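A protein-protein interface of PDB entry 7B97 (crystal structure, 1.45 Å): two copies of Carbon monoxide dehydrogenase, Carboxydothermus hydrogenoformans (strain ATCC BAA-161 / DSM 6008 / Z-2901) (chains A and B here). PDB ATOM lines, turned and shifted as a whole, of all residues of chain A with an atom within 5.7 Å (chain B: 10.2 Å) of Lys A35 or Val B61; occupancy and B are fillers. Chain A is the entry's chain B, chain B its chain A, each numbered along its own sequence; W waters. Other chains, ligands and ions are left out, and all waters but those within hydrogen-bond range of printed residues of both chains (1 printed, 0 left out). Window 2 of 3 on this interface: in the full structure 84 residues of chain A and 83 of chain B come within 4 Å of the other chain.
NH1 of Arg B56 sits at hydrogen-bond distance from O of Ile A36 (2.9 Å).
O of Asn B52 is in hydrogen-bond range of NH2 of Arg A37 (2.9 Å).
The side-chain amino group (NZ) of Lys A35 lies within hydrogen-bond range of the backbone carbonyl oxygen (O) of Val B61.
O of Pro B54 sits at hydrogen-bond distance from NH2 of Arg A37, at 2.7 Å.
O of Leu B65 sits at hydrogen-bond distance from NE2 of Gln A33 (3.3 Å).
The backbone NH (N) of Arg B56 sits at hydrogen-bond distance from the side-chain amide oxygen (OE1) of Gln A33, at 2.9 Å.
The backbone NH of Asn B58 sits at hydrogen-bond distance from the backbone carbonyl oxygen of Ala B63 (2.8 Å).
N of Lys B60 lies within hydrogen-bond range of OD1 of Asn B58 (2.9 Å).
The backbone NH (N) of Val B67 lies close to the side-chain sulfur (SG) of Cys B55, 3.6 Å away.
The side-chain carboxylate (OE2) of Glu A34 lies within salt-bridge range of the guanidinium group (NE) of Arg A37 (2.7 Å).
The side-chain amide nitrogen (ND2) of Asn B58 is in hydrogen-bond range of the side-chain hydroxyl (OH) of Tyr B40.
Among the printed residues, pairs that only touch across the chains: Gln A33 with Cys B55 (3.1 Å), Pro A32 with Gly B62 (3.4 Å), Ile A36 with Tyr B40 (3.7 Å), Gln A33 with Ala B63 (3.8 Å), Pro A32 with Ala B63 (3.8 Å), Gln A33 with Val B67 (3.8 Å) and Ile A36 with Asn B58 (3.9 Å).
Pro A32 touches just these residues of chain B: Gly B62 (3.4 Å) and Ala B63 (3.8 Å).
Of the printed residues of chain B, Gln A33 touches Cys B55 (3.1 Å), Arg B56 (2.9 Å), Ala B63 (3.8 Å), Leu B65 (3.3 Å) and Val B67 (3.8 Å).
Printed residues of chain A within 4 Å of Arg B56: Gln A33 and Ile A36.
Of the printed residues of chain A, Val B61 touches Lys A35.
Printed residues of chain A within 4 Å of Ala B63: Pro A32 and Gln A33.
The nearest residue of chain A that does not touch Val B61 is Ile A36 (4.1 Å).
Of the 15 printed residues of chain B, 11 touch a printed residue of chain A.
Hydrophobic or aromatic side chains of chain B that line the printed part of chain A: Tyr B40, Ala B63 and Val B67.
Of the 7 printed residues of chain A, 5 touch a printed residue of chain B.
Hydrophobic or aromatic side chains of chain A that line the printed part of chain B: Pro A32 and Ile A36.
Among the printed residues, 13 pairs touch across the chains.
Among the printed residues, no Asp or Glu carboxylate lies within 4 Å of a Lys or Arg side-chain nitrogen of the other chain.
No position is printed for both chains.
Of the 13 pairs that touch across the chains among the printed residues, none has its exchanged pair printed and touching as well.
Water W1 bridges O of Leu B65 (2.8 Å) and NE2 of Gln A33 (3.3 Å).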
ATOM      1  N   ASP A  31     -28.709 -18.229   0.831  1.00  0.00           N
ATOM      2  CA  ASP A  31     -30.165 -18.361   0.850  1.00  0.00           C
ATOM      3  C   ASP A  31     -30.625 -19.810   0.824  1.00  0.00           C
ATOM      4  O   ASP A  31     -31.549 -20.157   1.579  1.00  0.00           O
ATOM      5  CB  ASP A  31     -30.781 -17.559  -0.296  1.00  0.00           C
ATOM      6  CG  ASP A  31     -30.623 -16.059  -0.120  1.00  0.00           C
ATOM      7  OD1 ASP A  31     -30.533 -15.589   1.040  1.00  0.00           O
ATOM      8  OD2 ASP A  31     -30.604 -15.348  -1.156  1.00  0.00           O
ATOM      9  N   PRO A  32     -30.074 -20.689  -0.010  1.00  0.00           N
ATOM     10  CA  PRO A  32     -30.499 -22.097   0.073  1.00  0.00           C
ATOM     11  C   PRO A  32     -30.264 -22.701   1.438  1.00  0.00           C
ATOM     12  O   PRO A  32     -31.042 -23.550   1.883  1.00  0.00           O
ATOM     13  CB  PRO A  32     -29.678 -22.783  -1.026  1.00  0.00           C
ATOM     14  CG  PRO A  32     -29.313 -21.699  -1.966  1.00  0.00           C
ATOM     15  CD  PRO A  32     -29.184 -20.442  -1.156  1.00  0.00           C
ATOM     16  N   GLN A  33     -29.176 -22.321   2.102  1.00  0.00           N
ATOM     17  CA  GLN A  33     -28.897 -22.872   3.420  1.00  0.00           C
ATOM     18  C   GLN A  33     -29.997 -22.525   4.403  1.00  0.00           C
ATOM     19  O   GLN A  33     -30.286 -23.311   5.312  1.00  0.00           O
ATOM     20  CB  GLN A  33     -27.556 -22.351   3.929  1.00  0.00           C
ATOM     21  CG  GLN A  33     -26.334 -22.857   3.164  1.00  0.00           C
ATOM     22  CD  GLN A  33     -26.175 -24.366   3.251  1.00  0.00           C
ATOM     23  OE1 GLN A  33     -26.527 -24.970   4.261  1.00  0.00           O
ATOM     24  NE2 GLN A  33     -25.642 -24.981   2.193  1.00  0.00           N
ATOM     25  N   GLU A  34     -30.654 -21.367   4.212  1.00  0.00           N
ATOM     26  CA  GLU A  34     -31.697 -20.893   5.118  1.00  0.00           C
ATOM     27  C   GLU A  34     -32.965 -21.714   5.020  1.00  0.00           C
ATOM     28  O   GLU A  34     -33.843 -21.574   5.883  1.00  0.00           O
ATOM     29  CB  GLU A  34     -32.024 -19.434   4.831  1.00  0.00           C
ATOM     30  CG  GLU A  34     -30.898 -18.478   5.195  1.00  0.00           C
ATOM     31  CD  GLU A  34     -30.715 -18.290   6.696  1.00  0.00           C
ATOM     32  OE1 GLU A  34     -31.395 -17.424   7.264  1.00  0.00           O
ATOM     33  OE2 GLU A  34     -29.863 -18.971   7.300  1.00  0.00           O
ATOM     34  N   LYS A  35     -33.090 -22.551   4.003  1.00  0.00           N
ATOM     35  CA  LYS A  35     -34.274 -23.373   3.861  1.00  0.00           C
ATOM     36  C   LYS A  35     -34.260 -24.548   4.819  1.00  0.00           C
ATOM     37  O   LYS A  35     -35.326 -25.053   5.186  1.00  0.00           O
ATOM     38  CB  LYS A  35     -34.347 -23.922   2.430  1.00  0.00           C
ATOM     39  CG  LYS A  35     -34.571 -22.889   1.318  1.00  0.00           C
ATOM     40  CD  LYS A  35     -34.547 -23.622  -0.010  1.00  0.00           C
ATOM     41  CE  LYS A  35     -34.800 -22.736  -1.193  1.00  0.00           C
ATOM     42  NZ  LYS A  35     -34.761 -23.554  -2.447  1.00  0.00           N
ATOM     43  N   ILE A  36     -33.071 -25.024   5.202  1.00  0.00           N
ATOM     44  CA  ILE A  36     -32.965 -26.284   5.929  1.00  0.00           C
ATOM     45  C   ILE A  36     -31.975 -26.193   7.081  1.00  0.00           C
ATOM     46  O   ILE A  36     -31.338 -27.194   7.419  1.00  0.00           O
ATOM     47  CB  ILE A  36     -32.584 -27.446   4.983  1.00  0.00           C
ATOM     48  CG1 ILE A  36     -31.265 -27.135   4.266  1.00  0.00           C
ATOM     49  CG2 ILE A  36     -33.683 -27.730   3.952  1.00  0.00           C
ATOM     50  CD1 ILE A  36     -30.742 -28.295   3.398  1.00  0.00           C
ATOM     51  N   ARG A  37     -31.853 -25.028   7.721  1.00  0.00           N
ATOM     52  CA  ARG A  37     -30.885 -24.899   8.810  1.00  0.00           C
ATOM     53  C   ARG A  37     -31.186 -25.872   9.947  1.00  0.00           C
ATOM     54  O   ARG A  37     -32.337 -26.052  10.357  1.00  0.00           O
ATOM     55  CB  ARG A  37     -30.853 -23.483   9.380  1.00  0.00           C
ATOM     56  CG  ARG A  37     -30.352 -22.427   8.431  1.00  0.00           C
ATOM     57  CD  ARG A  37     -28.860 -22.496   8.202  1.00  0.00           C
ATOM     58  NE  ARG A  37     -28.415 -21.237   7.610  1.00  0.00           N
ATOM     59  CZ  ARG A  37     -27.152 -20.952   7.318  1.00  0.00           C
ATOM     60  NH1 ARG A  37     -26.831 -19.772   6.800  1.00  0.00           N
ATOM     61  NH2 ARG A  37     -26.219 -21.855   7.521  1.00  0.00           N
ATOM     62  N   TYR B  40     -27.919 -35.921   7.210  1.00  0.00           N
ATOM     63  CA  TYR B  40     -26.828 -35.123   6.660  1.00  0.00           C
ATOM     64  C   TYR B  40     -25.509 -35.490   7.323  1.00  0.00           C
ATOM     65  O   TYR B  40     -24.511 -35.756   6.648  1.00  0.00           O
ATOM     66  CB  TYR B  40     -27.112 -33.638   6.831  1.00  0.00           C
ATOM     67  CG  TYR B  40     -28.284 -33.152   6.036  1.00  0.00           C
ATOM     68  CD1 TYR B  40     -28.135 -32.718   4.713  1.00  0.00           C
ATOM     69  CD2 TYR B  40     -29.564 -33.182   6.578  1.00  0.00           C
ATOM     70  CE1 TYR B  40     -29.201 -32.291   3.979  1.00  0.00           C
ATOM     71  CE2 TYR B  40     -30.648 -32.754   5.841  1.00  0.00           C
ATOM     72  CZ  TYR B  40     -30.469 -32.304   4.535  1.00  0.00           C
ATOM     73  OH  TYR B  40     -31.553 -31.877   3.781  1.00  0.00           O
ATOM     74  N   ASN B  52     -21.037 -18.893   9.314  1.00  0.00           N
ATOM     75  CA  ASN B  52     -22.006 -18.896   8.208  1.00  0.00           C
ATOM     76  C   ASN B  52     -22.807 -20.189   8.156  1.00  0.00           C
ATOM     77  O   ASN B  52     -23.825 -20.250   7.468  1.00  0.00           O
ATOM     78  CB  ASN B  52     -21.328 -18.681   6.850  1.00  0.00           C
ATOM     79  CG  ASN B  52     -21.005 -17.229   6.565  1.00  0.00           C
ATOM     80  OD1 ASN B  52     -21.823 -16.346   6.746  1.00  0.00           O
ATOM     81  ND2 ASN B  52     -19.796 -16.987   6.079  1.00  0.00           N
ATOM     82  N   PRO B  54     -24.740 -23.449  10.516  1.00  0.00           N
ATOM     83  CA  PRO B  54     -24.399 -24.785  10.015  1.00  0.00           C
ATOM     84  C   PRO B  54     -24.859 -24.974   8.566  1.00  0.00           C
ATOM     85  O   PRO B  54     -25.936 -24.479   8.190  1.00  0.00           O
ATOM     86  CB  PRO B  54     -25.134 -25.720  10.969  1.00  0.00           C
ATOM     87  CG  PRO B  54     -26.310 -24.925  11.424  1.00  0.00           C
ATOM     88  CD  PRO B  54     -25.844 -23.490  11.493  1.00  0.00           C
ATOM     89  N   CYS B  55     -24.038 -25.619   7.755  1.00  0.00           N
ATOM     90  CA  CYS B  55     -24.354 -25.816   6.345  1.00  0.00           C
ATOM     91  C   CYS B  55     -24.679 -27.279   6.087  1.00  0.00           C
ATOM     92  O   CYS B  55     -24.212 -28.170   6.801  1.00  0.00           O
ATOM     93  CB  CYS B  55     -23.173 -25.410   5.456  1.00  0.00           C
ATOM     94  SG  CYS B  55     -22.920 -23.634   5.370  1.00  0.00           S
ATOM     95  N   ARG B  56     -25.433 -27.497   5.014  1.00  0.00           N
ATOM     96  CA  ARG B  56     -25.877 -28.810   4.553  1.00  0.00           C
ATOM     97  C   ARG B  56     -25.810 -28.812   3.036  1.00  0.00           C
ATOM     98  O   ARG B  56     -26.090 -27.792   2.398  1.00  0.00           O
ATOM     99  CB  ARG B  56     -27.320 -29.121   4.970  1.00  0.00           C
ATOM    100  CG  ARG B  56     -27.441 -29.437   6.442  1.00  0.00           C
ATOM    101  CD  ARG B  56     -28.880 -29.364   6.885  1.00  0.00           C
ATOM    102  NE  ARG B  56     -29.054 -30.159   8.085  1.00  0.00           N
ATOM    103  CZ  ARG B  56     -30.208 -30.467   8.635  1.00  0.00           C
ATOM    104  NH1 ARG B  56     -31.329 -29.989   8.128  1.00  0.00           N
ATOM    105  NH2 ARG B  56     -30.235 -31.265   9.690  1.00  0.00           N
ATOM    106  N   ILE B  57     -25.438 -29.944   2.459  1.00  0.00           N
ATOM    107  CA  ILE B  57     -25.544 -30.133   1.021  1.00  0.00           C
ATOM    108  C   ILE B  57     -26.847 -30.863   0.702  1.00  0.00           C
ATOM    109  O   ILE B  57     -27.069 -31.995   1.154  1.00  0.00           O
ATOM    110  CB  ILE B  57     -24.343 -30.912   0.456  1.00  0.00           C
ATOM    111  CG1 ILE B  57     -23.002 -30.256   0.838  1.00  0.00           C
ATOM    112  CG2 ILE B  57     -24.503 -31.045  -1.065  1.00  0.00           C
ATOM    113  CD1 ILE B  57     -22.850 -28.808   0.417  1.00  0.00           C
ATOM    114  N   ASN B  58     -27.687 -30.232  -0.123  1.00  0.00           N
ATOM    115  CA  ASN B  58     -28.910 -30.864  -0.622  1.00  0.00           C
ATOM    116  C   ASN B  58     -29.221 -30.191  -1.951  1.00  0.00           C
ATOM    117  O   ASN B  58     -29.766 -29.089  -1.978  1.00  0.00           O
ATOM    118  CB  ASN B  58     -30.054 -30.716   0.377  1.00  0.00           C
ATOM    119  CG  ASN B  58     -31.313 -31.464  -0.057  1.00  0.00           C
ATOM    120  OD1 ASN B  58     -31.549 -31.652  -1.248  1.00  0.00           O
ATOM    121  ND2 ASN B  58     -32.109 -31.906   0.908  1.00  0.00           N
ATOM    122  N   GLU B  59     -28.839 -30.843  -3.046  1.00  0.00           N
ATOM    123  CA  GLU B  59     -29.052 -30.234  -4.351  1.00  0.00           C
ATOM    124  C   GLU B  59     -30.531 -30.092  -4.665  1.00  0.00           C
ATOM    125  O   GLU B  59     -30.903 -29.189  -5.419  1.00  0.00           O
ATOM    126  CB  GLU B  59     -28.269 -30.990  -5.431  1.00  0.00           C
ATOM    127  CG  GLU B  59     -26.750 -30.782  -5.262  1.00  0.00           C
ATOM    128  CD  GLU B  59     -25.906 -31.573  -6.244  1.00  0.00           C
ATOM    129  OE1 GLU B  59     -26.391 -31.823  -7.367  1.00  0.00           O
ATOM    130  OE2 GLU B  59     -24.756 -31.932  -5.896  1.00  0.00           O
ATOM    131  N   LYS B  60     -31.384 -30.933  -4.084  1.00  0.00           N
ATOM    132  CA  LYS B  60     -32.808 -30.884  -4.415  1.00  0.00           C
ATOM    133  C   LYS B  60     -33.469 -29.588  -3.968  1.00  0.00           C
ATOM    134  O   LYS B  60     -34.502 -29.213  -4.527  1.00  0.00           O
ATOM    135  CB  LYS B  60     -33.553 -32.084  -3.827  1.00  0.00           C
ATOM    136  CG  LYS B  60     -33.546 -33.308  -4.734  1.00  0.00           C
ATOM    137  CD  LYS B  60     -33.922 -34.587  -3.986  1.00  0.00           C
ATOM    138  CE  LYS B  60     -33.851 -35.827  -4.898  1.00  0.00           C
ATOM    139  NZ  LYS B  60     -35.032 -35.914  -5.841  1.00  0.00           N
ATOM    140  N   VAL B  61     -32.904 -28.898  -2.978  1.00  0.00           N
ATOM    141  CA  VAL B  61     -33.385 -27.587  -2.559  1.00  0.00           C
ATOM    142  C   VAL B  61     -32.431 -26.468  -2.958  1.00  0.00           C
ATOM    143  O   VAL B  61     -32.577 -25.343  -2.480  1.00  0.00           O
ATOM    144  CB  VAL B  61     -33.704 -27.534  -1.055  1.00  0.00           C
ATOM    145  CG1 VAL B  61     -34.663 -28.662  -0.678  1.00  0.00           C
ATOM    146  CG2 VAL B  61     -32.422 -27.589  -0.227  1.00  0.00           C
ATOM    147  N   GLY B  62     -31.450 -26.746  -3.812  1.00  0.00           N
ATOM    148  CA  GLY B  62     -30.543 -25.713  -4.279  1.00  0.00           C
ATOM    149  C   GLY B  62     -29.307 -25.487  -3.436  1.00  0.00           C
ATOM    150  O   GLY B  62     -28.540 -24.559  -3.730  1.00  0.00           O
ATOM    151  N   ALA B  63     -29.081 -26.296  -2.404  1.00  0.00           N
ATOM    152  CA  ALA B  63     -27.920 -26.126  -1.535  1.00  0.00           C
ATOM    153  C   ALA B  63     -26.802 -27.039  -2.034  1.00  0.00           C
ATOM    154  O   ALA B  63     -26.530 -28.104  -1.488  1.00  0.00           O
ATOM    155  CB  ALA B  63     -28.313 -26.403  -0.086  1.00  0.00           C
ATOM    156  N   THR B  64     -26.138 -26.593  -3.102  1.00  0.00           N
ATOM    157  CA  THR B  64     -25.121 -27.408  -3.751  1.00  0.00           C
ATOM    158  C   THR B  64     -23.759 -27.272  -3.095  1.00  0.00           C
ATOM    159  O   THR B  64     -22.972 -28.238  -3.086  1.00  0.00           O
ATOM    160  CB  THR B  64     -24.996 -27.004  -5.218  1.00  0.00           C
ATOM    161  OG1 THR B  64     -26.221 -27.307  -5.886  1.00  0.00           O
ATOM    162  CG2 THR B  64     -23.829 -27.756  -5.880  1.00  0.00           C
ATOM    163  N   LEU B  65     -23.468 -26.087  -2.570  1.00  0.00           N
ATOM    164  CA  LEU B  65     -22.216 -25.783  -1.912  1.00  0.00           C
ATOM    165  C   LEU B  65     -22.505 -25.139  -0.570  1.00  0.00           C
ATOM    166  O   LEU B  65     -23.572 -24.545  -0.353  1.00  0.00           O
ATOM    167  CB  LEU B  65     -21.413 -24.798  -2.743  1.00  0.00           C
ATOM    168  CG  LEU B  65     -21.062 -25.261  -4.161  1.00  0.00           C
ATOM    169  CD1 LEU B  65     -20.394 -24.123  -4.935  1.00  0.00           C
ATOM    170  CD2 LEU B  65     -20.168 -26.500  -4.204  1.00  0.00           C
ATOM    171  N   VAL B  67     -21.797 -22.157   2.278  1.00  0.00           N
ATOM    172  CA  VAL B  67     -21.797 -20.713   2.025  1.00  0.00           C
ATOM    173  C   VAL B  67     -20.444 -20.273   1.475  1.00  0.00           C
ATOM    174  O   VAL B  67     -20.367 -19.452   0.547  1.00  0.00           O
ATOM    175  CB  VAL B  67     -22.182 -19.921   3.280  1.00  0.00           C
ATOM    176  CG1 VAL B  67     -22.027 -18.437   3.000  1.00  0.00           C
ATOM    177  CG2 VAL B  67     -23.611 -20.241   3.685  1.00  0.00           C
HETATM  178  O   HOH W   1     -25.910 -23.063  -0.538  1.00  0.00           O
